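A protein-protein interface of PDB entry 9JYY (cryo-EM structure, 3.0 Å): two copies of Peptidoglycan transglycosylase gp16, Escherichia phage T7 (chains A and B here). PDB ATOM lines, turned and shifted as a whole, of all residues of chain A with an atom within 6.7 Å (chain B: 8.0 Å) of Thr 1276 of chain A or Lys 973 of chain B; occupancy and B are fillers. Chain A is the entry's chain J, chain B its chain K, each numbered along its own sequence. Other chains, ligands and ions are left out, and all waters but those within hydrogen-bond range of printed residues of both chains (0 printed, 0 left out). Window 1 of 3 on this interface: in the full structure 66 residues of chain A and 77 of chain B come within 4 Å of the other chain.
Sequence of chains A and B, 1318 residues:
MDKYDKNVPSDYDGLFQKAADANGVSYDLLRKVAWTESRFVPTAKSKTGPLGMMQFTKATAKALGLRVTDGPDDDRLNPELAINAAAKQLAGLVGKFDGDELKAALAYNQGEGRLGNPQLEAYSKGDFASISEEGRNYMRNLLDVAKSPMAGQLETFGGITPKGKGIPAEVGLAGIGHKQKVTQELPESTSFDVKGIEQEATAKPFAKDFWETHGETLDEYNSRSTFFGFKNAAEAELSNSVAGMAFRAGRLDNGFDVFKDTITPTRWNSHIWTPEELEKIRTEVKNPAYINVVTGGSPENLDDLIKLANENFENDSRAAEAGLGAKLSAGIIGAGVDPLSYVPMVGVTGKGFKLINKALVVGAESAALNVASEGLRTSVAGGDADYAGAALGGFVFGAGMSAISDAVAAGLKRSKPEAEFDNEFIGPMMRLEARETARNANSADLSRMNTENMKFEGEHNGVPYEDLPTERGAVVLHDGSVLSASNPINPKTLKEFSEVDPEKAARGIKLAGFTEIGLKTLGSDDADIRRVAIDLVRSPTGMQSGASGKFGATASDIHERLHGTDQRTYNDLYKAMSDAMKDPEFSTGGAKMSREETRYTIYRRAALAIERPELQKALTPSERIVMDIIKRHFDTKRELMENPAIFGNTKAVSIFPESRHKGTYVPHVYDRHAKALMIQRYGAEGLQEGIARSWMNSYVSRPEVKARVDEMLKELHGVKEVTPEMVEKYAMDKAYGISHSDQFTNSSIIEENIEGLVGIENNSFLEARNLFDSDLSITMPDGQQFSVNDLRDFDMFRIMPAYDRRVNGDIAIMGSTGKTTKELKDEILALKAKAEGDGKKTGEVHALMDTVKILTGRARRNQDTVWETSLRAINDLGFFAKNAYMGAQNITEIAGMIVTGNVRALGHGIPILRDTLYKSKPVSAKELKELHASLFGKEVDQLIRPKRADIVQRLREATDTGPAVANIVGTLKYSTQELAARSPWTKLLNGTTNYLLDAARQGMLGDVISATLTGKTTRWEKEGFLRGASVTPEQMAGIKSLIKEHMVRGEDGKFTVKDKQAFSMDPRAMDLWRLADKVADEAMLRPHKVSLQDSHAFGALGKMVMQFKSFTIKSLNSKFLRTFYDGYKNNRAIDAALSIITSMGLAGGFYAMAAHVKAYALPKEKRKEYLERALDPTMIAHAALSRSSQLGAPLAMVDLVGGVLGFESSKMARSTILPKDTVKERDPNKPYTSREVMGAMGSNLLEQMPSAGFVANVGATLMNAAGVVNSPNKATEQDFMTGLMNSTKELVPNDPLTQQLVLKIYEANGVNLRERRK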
ATOM      1  N   ARG A 568     -16.755 -24.534   4.224  1.00  0.00           N
ATOM      2  CA  ARG A 568     -16.110 -25.799   3.893  1.00  0.00           C
ATOM      3  C   ARG A 568     -16.860 -26.974   4.498  1.00  0.00           C
ATOM      4  O   ARG A 568     -17.097 -27.987   3.827  1.00  0.00           O
ATOM      5  CB  ARG A 568     -14.659 -25.797   4.359  1.00  0.00           C
ATOM      6  CG  ARG A 568     -13.832 -24.693   3.744  1.00  0.00           C
ATOM      7  CD  ARG A 568     -12.440 -24.658   4.320  1.00  0.00           C
ATOM      8  NE  ARG A 568     -11.765 -25.943   4.203  1.00  0.00           N
ATOM      9  CZ  ARG A 568     -10.599 -26.223   4.766  1.00  0.00           C
ATOM     10  NH1 ARG A 568      -9.959 -25.331   5.502  1.00  0.00           N
ATOM     11  NH2 ARG A 568     -10.063 -27.425   4.586  1.00  0.00           N
ATOM     12  N   ASP A 876     -11.372 -14.062 -10.927  1.00  0.00           N
ATOM     13  CA  ASP A 876     -10.076 -14.367 -10.325  1.00  0.00           C
ATOM     14  C   ASP A 876      -9.518 -15.678 -10.875  1.00  0.00           C
ATOM     15  O   ASP A 876      -8.320 -15.786 -11.175  1.00  0.00           O
ATOM     16  CB  ASP A 876     -10.213 -14.420  -8.805  1.00  0.00           C
ATOM     17  CG  ASP A 876      -8.875 -14.516  -8.092  1.00  0.00           C
ATOM     18  OD1 ASP A 876      -7.831 -14.573  -8.764  1.00  0.00           O
ATOM     19  OD2 ASP A 876      -8.865 -14.531  -6.846  1.00  0.00           O
ATOM     20  N   GLU A1247       4.899 -21.132   6.910  1.00  0.00           N
ATOM     21  CA  GLU A1247       3.728 -21.869   7.374  1.00  0.00           C
ATOM     22  C   GLU A1247       4.033 -23.346   7.573  1.00  0.00           C
ATOM     23  O   GLU A1247       4.494 -24.029   6.654  1.00  0.00           O
ATOM     24  CB  GLU A1247       2.584 -21.720   6.377  1.00  0.00           C
ATOM     25  CG  GLU A1247       2.278 -20.299   5.972  1.00  0.00           C
ATOM     26  CD  GLU A1247       0.904 -20.174   5.353  1.00  0.00           C
ATOM     27  OE1 GLU A1247       0.659 -20.824   4.316  1.00  0.00           O
ATOM     28  OE2 GLU A1247       0.065 -19.433   5.906  1.00  0.00           O
ATOM     29  N   PRO A1272      -6.947 -20.025   6.971  1.00  0.00           N
ATOM     30  CA  PRO A1272      -6.890 -18.659   6.443  1.00  0.00           C
ATOM     31  C   PRO A1272      -8.276 -18.043   6.365  1.00  0.00           C
ATOM     32  O   PRO A1272      -9.280 -18.745   6.231  1.00  0.00           O
ATOM     33  CB  PRO A1272      -6.289 -18.845   5.050  1.00  0.00           C
ATOM     34  CG  PRO A1272      -6.628 -20.244   4.689  1.00  0.00           C
ATOM     35  CD  PRO A1272      -6.568 -21.022   5.958  1.00  0.00           C
ATOM     36  N   ASN A1273      -8.325 -16.715   6.452  1.00  0.00           N
ATOM     37  CA  ASN A1273      -9.614 -16.037   6.399  1.00  0.00           C
ATOM     38  C   ASN A1273     -10.145 -15.956   4.972  1.00  0.00           C
ATOM     39  O   ASN A1273     -11.361 -15.989   4.754  1.00  0.00           O
ATOM     40  CB  ASN A1273      -9.507 -14.649   7.025  1.00  0.00           C
ATOM     41  CG  ASN A1273      -8.271 -13.912   6.595  1.00  0.00           C
ATOM     42  OD1 ASN A1273      -7.575 -14.330   5.672  1.00  0.00           O
ATOM     43  ND2 ASN A1273      -7.987 -12.802   7.264  1.00  0.00           N
ATOM     44  N   LYS A1274      -9.259 -15.840   3.990  1.00  0.00           N
ATOM     45  CA  LYS A1274      -9.688 -15.832   2.598  1.00  0.00           C
ATOM     46  C   LYS A1274     -10.076 -17.231   2.137  1.00  0.00           C
ATOM     47  O   LYS A1274      -9.456 -18.224   2.524  1.00  0.00           O
ATOM     48  CB  LYS A1274      -8.579 -15.282   1.706  1.00  0.00           C
ATOM     49  CG  LYS A1274      -8.716 -13.807   1.383  1.00  0.00           C
ATOM     50  CD  LYS A1274      -7.402 -13.225   0.890  1.00  0.00           C
ATOM     51  CE  LYS A1274      -6.687 -14.169  -0.052  1.00  0.00           C
ATOM     52  NZ  LYS A1274      -7.487 -14.399  -1.274  1.00  0.00           N
ATOM     53  N   ALA A1275     -11.105 -17.303   1.298  1.00  0.00           N
ATOM     54  CA  ALA A1275     -11.530 -18.578   0.738  1.00  0.00           C
ATOM     55  C   ALA A1275     -10.620 -18.979  -0.411  1.00  0.00           C
ATOM     56  O   ALA A1275     -10.307 -18.172  -1.286  1.00  0.00           O
ATOM     57  CB  ALA A1275     -12.976 -18.493   0.256  1.00  0.00           C
ATOM     58  N   THR A1276     -10.195 -20.235  -0.410  1.00  0.00           N
ATOM     59  CA  THR A1276      -9.242 -20.665  -1.413  1.00  0.00           C
ATOM     60  C   THR A1276      -9.956 -21.039  -2.707  1.00  0.00           C
ATOM     61  O   THR A1276     -11.185 -21.063  -2.786  1.00  0.00           O
ATOM     62  CB  THR A1276      -8.419 -21.846  -0.915  1.00  0.00           C
ATOM     63  OG1 THR A1276      -9.268 -22.981  -0.744  1.00  0.00           O
ATOM     64  CG2 THR A1276      -7.783 -21.513   0.417  1.00  0.00           C
ATOM     65  N   GLU A1277      -9.158 -21.319  -3.737  1.00  0.00           N
ATOM     66  CA  GLU A1277      -9.724 -21.639  -5.041  1.00  0.00           C
ATOM     67  C   GLU A1277     -10.534 -22.929  -4.997  1.00  0.00           C
ATOM     68  O   GLU A1277     -11.622 -23.004  -5.580  1.00  0.00           O
ATOM     69  CB  GLU A1277      -8.607 -21.705  -6.090  1.00  0.00           C
ATOM     70  CG  GLU A1277      -7.807 -23.005  -6.153  1.00  0.00           C
ATOM     71  CD  GLU A1277      -6.829 -23.153  -4.998  1.00  0.00           C
ATOM     72  OE1 GLU A1277      -6.123 -24.181  -4.938  1.00  0.00           O
ATOM     73  OE2 GLU A1277      -6.755 -22.238  -4.153  1.00  0.00           O
ATOM     74  N   GLN A1278     -10.033 -23.951  -4.299  1.00  0.00           N
ATOM     75  CA  GLN A1278     -10.745 -25.221  -4.273  1.00  0.00           C
ATOM     76  C   GLN A1278     -12.035 -25.109  -3.476  1.00  0.00           C
ATOM     77  O   GLN A1278     -13.037 -25.739  -3.825  1.00  0.00           O
ATOM     78  CB  GLN A1278      -9.846 -26.339  -3.734  1.00  0.00           C
ATOM     79  CG  GLN A1278      -9.743 -26.463  -2.230  1.00  0.00           C
ATOM     80  CD  GLN A1278      -8.527 -25.766  -1.673  1.00  0.00           C
ATOM     81  OE1 GLN A1278      -8.164 -24.682  -2.117  1.00  0.00           O
ATOM     82  NE2 GLN A1278      -7.881 -26.392  -0.700  1.00  0.00           N
ATOM     83  N   ASP A1279     -12.042 -24.296  -2.418  1.00  0.00           N
ATOM     84  CA  ASP A1279     -13.282 -24.073  -1.682  1.00  0.00           C
ATOM     85  C   ASP A1279     -14.349 -23.469  -2.575  1.00  0.00           C
ATOM     86  O   ASP A1279     -15.467 -23.991  -2.658  1.00  0.00           O
ATOM     87  CB  ASP A1279     -13.041 -23.170  -0.475  1.00  0.00           C
ATOM     88  CG  ASP A1279     -11.893 -23.637   0.380  1.00  0.00           C
ATOM     89  OD1 ASP A1279     -11.449 -24.788   0.202  1.00  0.00           O
ATOM     90  OD2 ASP A1279     -11.429 -22.853   1.233  1.00  0.00           O
ATOM     91  N   PHE A1280     -14.023 -22.373  -3.265  1.00  0.00           N
ATOM     92  CA  PHE A1280     -15.005 -21.766  -4.151  1.00  0.00           C
ATOM     93  C   PHE A1280     -15.442 -22.736  -5.229  1.00  0.00           C
ATOM     94  O   PHE A1280     -16.619 -22.776  -5.595  1.00  0.00           O
ATOM     95  CB  PHE A1280     -14.467 -20.508  -4.819  1.00  0.00           C
ATOM     96  CG  PHE A1280     -15.285 -20.092  -6.004  1.00  0.00           C
ATOM     97  CD1 PHE A1280     -16.570 -19.611  -5.832  1.00  0.00           C
ATOM     98  CD2 PHE A1280     -14.803 -20.244  -7.290  1.00  0.00           C
ATOM     99  CE1 PHE A1280     -17.342 -19.259  -6.912  1.00  0.00           C
ATOM    100  CE2 PHE A1280     -15.574 -19.894  -8.373  1.00  0.00           C
ATOM    101  CZ  PHE A1280     -16.843 -19.400  -8.184  1.00  0.00           C
ATOM    102  N   MET A1281     -14.509 -23.509  -5.772  1.00  0.00           N
ATOM    103  CA  MET A1281     -14.859 -24.331  -6.917  1.00  0.00           C
ATOM    104  C   MET A1281     -15.764 -25.483  -6.508  1.00  0.00           C
ATOM    105  O   MET A1281     -16.759 -25.769  -7.185  1.00  0.00           O
ATOM    106  CB  MET A1281     -13.599 -24.837  -7.607  1.00  0.00           C
ATOM    107  CG  MET A1281     -13.094 -23.866  -8.655  1.00  0.00           C
ATOM    108  SD  MET A1281     -14.106 -23.870 -10.135  1.00  0.00           S
ATOM    109  CE  MET A1281     -14.128 -25.606 -10.489  1.00  0.00           C
ATOM    110  N   GLN B 784      -1.523 -11.346   9.547  1.00  0.00           N
ATOM    111  CA  GLN B 784      -1.078 -12.613   9.019  1.00  0.00           C
ATOM    112  C   GLN B 784      -0.765 -13.532  10.194  1.00  0.00           C
ATOM    113  O   GLN B 784      -0.425 -13.081  11.288  1.00  0.00           O
ATOM    114  CB  GLN B 784       0.132 -12.435   8.100  1.00  0.00           C
ATOM    115  CG  GLN B 784      -0.331 -12.102   6.681  1.00  0.00           C
ATOM    116  CD  GLN B 784      -0.606 -13.308   5.826  1.00  0.00           C
ATOM    117  OE1 GLN B 784       0.286 -13.940   5.271  1.00  0.00           O
ATOM    118  NE2 GLN B 784      -1.888 -13.620   5.696  1.00  0.00           N
ATOM    119  N   GLN B 785      -0.931 -14.827   9.984  1.00  0.00           N
ATOM    120  CA  GLN B 785      -0.947 -15.788  11.076  1.00  0.00           C
ATOM    121  C   GLN B 785       0.429 -16.376  11.320  1.00  0.00           C
ATOM    122  O   GLN B 785       1.122 -16.757  10.373  1.00  0.00           O
ATOM    123  CB  GLN B 785      -1.927 -16.912  10.781  1.00  0.00           C
ATOM    124  CG  GLN B 785      -3.311 -16.423  10.532  1.00  0.00           C
ATOM    125  CD  GLN B 785      -4.333 -17.389  11.040  1.00  0.00           C
ATOM    126  OE1 GLN B 785      -4.376 -17.696  12.232  1.00  0.00           O
ATOM    127  NE2 GLN B 785      -5.164 -17.895  10.139  1.00  0.00           N
ATOM    128  N   GLY B 962       3.320 -14.366 -10.209  1.00  0.00           N
ATOM    129  CA  GLY B 962       2.023 -14.939  -9.947  1.00  0.00           C
ATOM    130  C   GLY B 962       1.628 -14.909  -8.484  1.00  0.00           C
ATOM    131  O   GLY B 962       0.538 -14.447  -8.128  1.00  0.00           O
ATOM    132  N   PRO B 963       2.495 -15.427  -7.608  1.00  0.00           N
ATOM    133  CA  PRO B 963       2.207 -15.330  -6.169  1.00  0.00           C
ATOM    134  C   PRO B 963       2.003 -13.906  -5.686  1.00  0.00           C
ATOM    135  O   PRO B 963       1.081 -13.653  -4.902  1.00  0.00           O
ATOM    136  CB  PRO B 963       3.443 -15.965  -5.528  1.00  0.00           C
ATOM    137  CG  PRO B 963       3.942 -16.917  -6.536  1.00  0.00           C
ATOM    138  CD  PRO B 963       3.553 -16.410  -7.892  1.00  0.00           C
ATOM    139  N   ALA B 966      -1.371 -12.544  -6.999  1.00  0.00           N
ATOM    140  CA  ALA B 966      -2.484 -13.185  -6.311  1.00  0.00           C
ATOM    141  C   ALA B 966      -2.610 -12.688  -4.880  1.00  0.00           C
ATOM    142  O   ALA B 966      -3.722 -12.509  -4.372  1.00  0.00           O
ATOM    143  CB  ALA B 966      -2.316 -14.698  -6.333  1.00  0.00           C
ATOM    144  N   ASN B 967      -1.480 -12.468  -4.209  1.00  0.00           N
ATOM    145  CA  ASN B 967      -1.528 -12.021  -2.824  1.00  0.00           C
ATOM    146  C   ASN B 967      -2.054 -10.598  -2.721  1.00  0.00           C
ATOM    147  O   ASN B 967      -2.720 -10.243  -1.742  1.00  0.00           O
ATOM    148  CB  ASN B 967      -0.144 -12.139  -2.192  1.00  0.00           C
ATOM    149  CG  ASN B 967       0.240 -13.573  -1.914  1.00  0.00           C
ATOM    150  OD1 ASN B 967      -0.570 -14.356  -1.422  1.00  0.00           O
ATOM    151  ND2 ASN B 967       1.476 -13.930  -2.237  1.00  0.00           N
ATOM    152  N   GLY B 970      -5.730 -10.782  -5.860  1.00  0.00           N
ATOM    153  CA  GLY B 970      -6.656 -11.895  -5.986  1.00  0.00           C
ATOM    154  C   GLY B 970      -7.634 -11.968  -4.828  1.00  0.00           C
ATOM    155  O   GLY B 970      -7.301 -11.659  -3.681  1.00  0.00           O
ATOM    156  N   THR B 971      -8.862 -12.377  -5.140  1.00  0.00           N
ATOM    157  CA  THR B 971      -9.892 -12.601  -4.137  1.00  0.00           C
ATOM    158  C   THR B 971      -9.923 -14.033  -3.622  1.00  0.00           C
ATOM    159  O   THR B 971     -10.539 -14.287  -2.582  1.00  0.00           O
ATOM    160  CB  THR B 971     -11.268 -12.243  -4.705  1.00  0.00           C
ATOM    161  OG1 THR B 971     -11.601 -13.152  -5.759  1.00  0.00           O
ATOM    162  CG2 THR B 971     -11.263 -10.823  -5.252  1.00  0.00           C
ATOM    163  N   LEU B 972      -9.284 -14.968  -4.316  1.00  0.00           N
ATOM    164  CA  LEU B 972      -9.137 -16.340  -3.857  1.00  0.00           C
ATOM    165  C   LEU B 972      -7.698 -16.541  -3.419  1.00  0.00           C
ATOM    166  O   LEU B 972      -6.784 -15.934  -3.982  1.00  0.00           O
ATOM    167  CB  LEU B 972      -9.502 -17.350  -4.946  1.00  0.00           C
ATOM    168  CG  LEU B 972     -10.954 -17.348  -5.429  1.00  0.00           C
ATOM    169  CD1 LEU B 972     -11.149 -18.403  -6.492  1.00  0.00           C
ATOM    170  CD2 LEU B 972     -11.916 -17.557  -4.276  1.00  0.00           C
ATOM    171  N   LYS B 973      -7.500 -17.372  -2.398  1.00  0.00           N
ATOM    172  CA  LYS B 973      -6.203 -17.411  -1.732  1.00  0.00           C
ATOM    173  C   LYS B 973      -5.125 -17.995  -2.634  1.00  0.00           C
ATOM    174  O   LYS B 973      -4.027 -17.438  -2.744  1.00  0.00           O
ATOM    175  CB  LYS B 973      -6.298 -18.201  -0.432  1.00  0.00           C
ATOM    176  CG  LYS B 973      -4.978 -18.276   0.304  1.00  0.00           C
ATOM    177  CD  LYS B 973      -4.990 -19.330   1.384  1.00  0.00           C
ATOM    178  CE  LYS B 973      -3.891 -19.067   2.390  1.00  0.00           C
ATOM    179  NZ  LYS B 973      -3.958 -17.672   2.899  1.00  0.00           N
ATOM    180  N   TYR B 974      -5.423 -19.116  -3.289  1.00  0.00           N
ATOM    181  CA  TYR B 974      -4.419 -19.896  -4.003  1.00  0.00           C
ATOM    182  C   TYR B 974      -3.290 -20.273  -3.061  1.00  0.00           C
ATOM    183  O   TYR B 974      -3.453 -20.227  -1.838  1.00  0.00           O
ATOM    184  CB  TYR B 974      -3.878 -19.136  -5.213  1.00  0.00           C
ATOM    185  CG  TYR B 974      -4.918 -18.920  -6.273  1.00  0.00           C
ATOM    186  CD1 TYR B 974      -5.420 -19.984  -6.998  1.00  0.00           C
ATOM    187  CD2 TYR B 974      -5.411 -17.658  -6.536  1.00  0.00           C
ATOM    188  CE1 TYR B 974      -6.375 -19.795  -7.960  1.00  0.00           C
ATOM    189  CE2 TYR B 974      -6.370 -17.463  -7.496  1.00  0.00           C
ATOM    190  CZ  TYR B 974      -6.848 -18.535  -8.204  1.00  0.00           C
ATOM    191  OH  TYR B 974      -7.804 -18.345  -9.165  1.00  0.00           O
ATOM    192  N   SER B 975      -2.147 -20.657  -3.611  1.00  0.00           N
ATOM    193  CA  SER B 975      -1.035 -21.078  -2.778  1.00  0.00           C
ATOM    194  C   SER B 975       0.254 -20.947  -3.563  1.00  0.00           C
ATOM    195  O   SER B 975       0.308 -21.264  -4.751  1.00  0.00           O
ATOM    196  CB  SER B 975      -1.206 -22.521  -2.299  1.00  0.00           C
ATOM    197  OG  SER B 975      -0.187 -22.877  -1.389  1.00  0.00           O
ATOM    198  N   THR B 976       1.289 -20.465  -2.892  1.00  0.00           N
ATOM    199  CA  THR B 976       2.621 -20.613  -3.440  1.00  0.00           C
ATOM    200  C   THR B 976       2.947 -22.097  -3.519  1.00  0.00           C
ATOM    201  O   THR B 976       2.659 -22.855  -2.594  1.00  0.00           O
ATOM    202  CB  THR B 976       3.641 -19.883  -2.576  1.00  0.00           C
ATOM    203  OG1 THR B 976       3.465 -20.266  -1.208  1.00  0.00           O
ATOM    204  CG2 THR B 976       3.443 -18.384  -2.695  1.00  0.00           C
ATOM    205  N   GLU B 978       1.563 -23.385  -6.132  1.00  0.00           N
ATOM    206  CA  GLU B 978       0.495 -23.569  -7.106  1.00  0.00           C
ATOM    207  C   GLU B 978       0.584 -22.518  -8.200  1.00  0.00           C
ATOM    208  O   GLU B 978       0.264 -22.807  -9.356  1.00  0.00           O
ATOM    209  CB  GLU B 978      -0.877 -23.516  -6.428  1.00  0.00           C
ATOM    210  CG  GLU B 978      -1.101 -24.602  -5.415  1.00  0.00           C
ATOM    211  CD  GLU B 978      -2.564 -24.923  -5.232  1.00  0.00           C
ATOM    212  OE1 GLU B 978      -3.294 -24.083  -4.667  1.00  0.00           O
ATOM    213  OE2 GLU B 978      -2.982 -26.020  -5.649  1.00  0.00           O
ATOM    214  N   LEU B 979       0.996 -21.302  -7.859  1.00  0.00           N
ATOM    215  CA  LEU B 979       1.129 -20.258  -8.863  1.00  0.00           C
ATOM    216  C   LEU B 979       2.581 -20.081  -9.278  1.00  0.00           C
ATOM    217  O   LEU B 979       2.891 -19.243 -10.132  1.00  0.00           O
ATOM    218  CB  LEU B 979       0.549 -18.959  -8.320  1.00  0.00           C
ATOM    219  CG  LEU B 979      -0.958 -19.077  -8.094  1.00  0.00           C
ATOM    220  CD1 LEU B 979      -1.532 -17.761  -7.676  1.00  0.00           C
ATOM    221  CD2 LEU B 979      -1.649 -19.580  -9.343  1.00  0.00           C
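No position is printed for both chains.
N of Thr 971 of chain B is in hydrogen-bond range of OD2 of Asp 876 of chain A, at 2.7 Å.
N of Leu 972 of chain B is in hydrogen-bond range of OD2 of Asp 876 of chain A (2.6 Å).
The backbone carbonyl oxygen (O) of Asp 876 of chain A lies within hydrogen-bond range of the side-chain hydroxyl (OH) of Tyr 974 of chain B.
The backbone carbonyl oxygen (O) of Thr 971 of chain B sits at hydrogen-bond distance from the side-chain amino group (NZ) of Lys 1274 of chain A, 3.3 Å away.
NZ of Lys 1274 of chain A sits close to O of Leu 972 of chain B, at 3.2 Å.
The backbone carbonyl oxygen (O) of Ala 1275 of chain A lies within hydrogen-bond range of the backbone NH (N) of Lys 973 of chain B.
NZ of Lys 1274 of chain A sits close to N of Lys 973 of chain B, at 3.2 Å.
The side-chain carboxylate of Glu 978 of chain B sits close to the side-chain carboxylate of Glu 1277 of chain A (2.8 Å).
Arg 568 of chain A touches none of the printed residues of chain B.
Of the printed residues of chain B, Asp 876 of chain A touches Gly 970 (3.5 Å), Thr 971 (2.7 Å), Leu 972 (2.6 Å) and Tyr 974 (3.3 Å).
Printed residues of chain B within 4 Å of Lys 1274 of chain A: Gly 970 (3.7 Å), Thr 971 (3.3 Å), Leu 972 (3.0 Å) and Lys 973 (3.2 Å).
Of chain B, only Leu 972 and Lys 973 come within 4 Å of Ala 1275 of chain A.
Of chain B, only Leu 972 and Lys 973 come within 4 Å of Thr 1276 of chain A.
Pro 963 of chain B touches none of the printed residues of chain A.
Of the printed residues of chain A, Thr 971 of chain B touches Asp 876 (2.7 Å) and Lys 1274 (3.3 Å).
Lys 973 of chain B touches four residues of chain A.
Printed residues of chain A within 4 Å of Tyr 974 of chain B: Asp 876 (3.3 Å) and Glu 1277 (3.3 Å).
The nearest printed residue of chain A that does not touch Tyr 974 of chain B is Thr 1276 of chain A (4.5 Å).
Hydrophobic or aromatic side chains of chain A that line the printed part of chain B: Pro 1272 and Phe 1280.
Of the 15 printed residues of chain B, 6 touch a printed residue of chain A.
Printed residues of chain B that touch a printed residue of chain A: Gly 970, Thr 971, Leu 972, Lys 973, Tyr 974 and Glu 978.
Hydrophobic or aromatic side chains of chain B that line the printed part of chain A: Leu 972 and Tyr 974.
Among the printed residues, 17 pairs touch across the chains.
Among the printed residues, no Asp or Glu carboxylate lies within 4 Å of a Lys or Arg side-chain nitrogen of the other chain.
Gly 970 of chain B touches Asp 876 of chain A.
Pro 1272 of chain A touches Lys 973 of chain B.
Gly 970 of chain B touches Lys 1274 of chain A.
Leu 972 of chain B touches Ala 1275 of chain A.
O of Thr 1276 of chain A touches CD2 of Leu 972 of chain B, 3.9 Å away.
CG2 of Thr 1276 of chain A touches CD of Lys 973 of chain B, at 3.7 Å.
Glu 1277 of chain A touches Leu 972 of chain B (CA to CD1, 3.8 Å).
Glu 1277 of chain A touches Tyr 974 of chain B (OE2 to CA, 3.3 Å).
CD2 of Leu 972 of chain B touches CB of Phe 1280 of chain A (3.9 Å).
The side-chain amide oxygen (OE1) of Gln 1278 of chain A sits at hydrogen-bond distance from the side-chain hydroxyl (OG1) of Thr 1276 of chain A (2.4 Å).
The side-chain carboxylate (OD2) of Asp 1279 of chain A sits close to the side-chain hydroxyl (OG1) of Thr 1276 of chain A (2.9 Å).
OE2 of Glu 1277 of chain A sits close to OE1 of Gln 1278 of chain A (3.5 Å).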
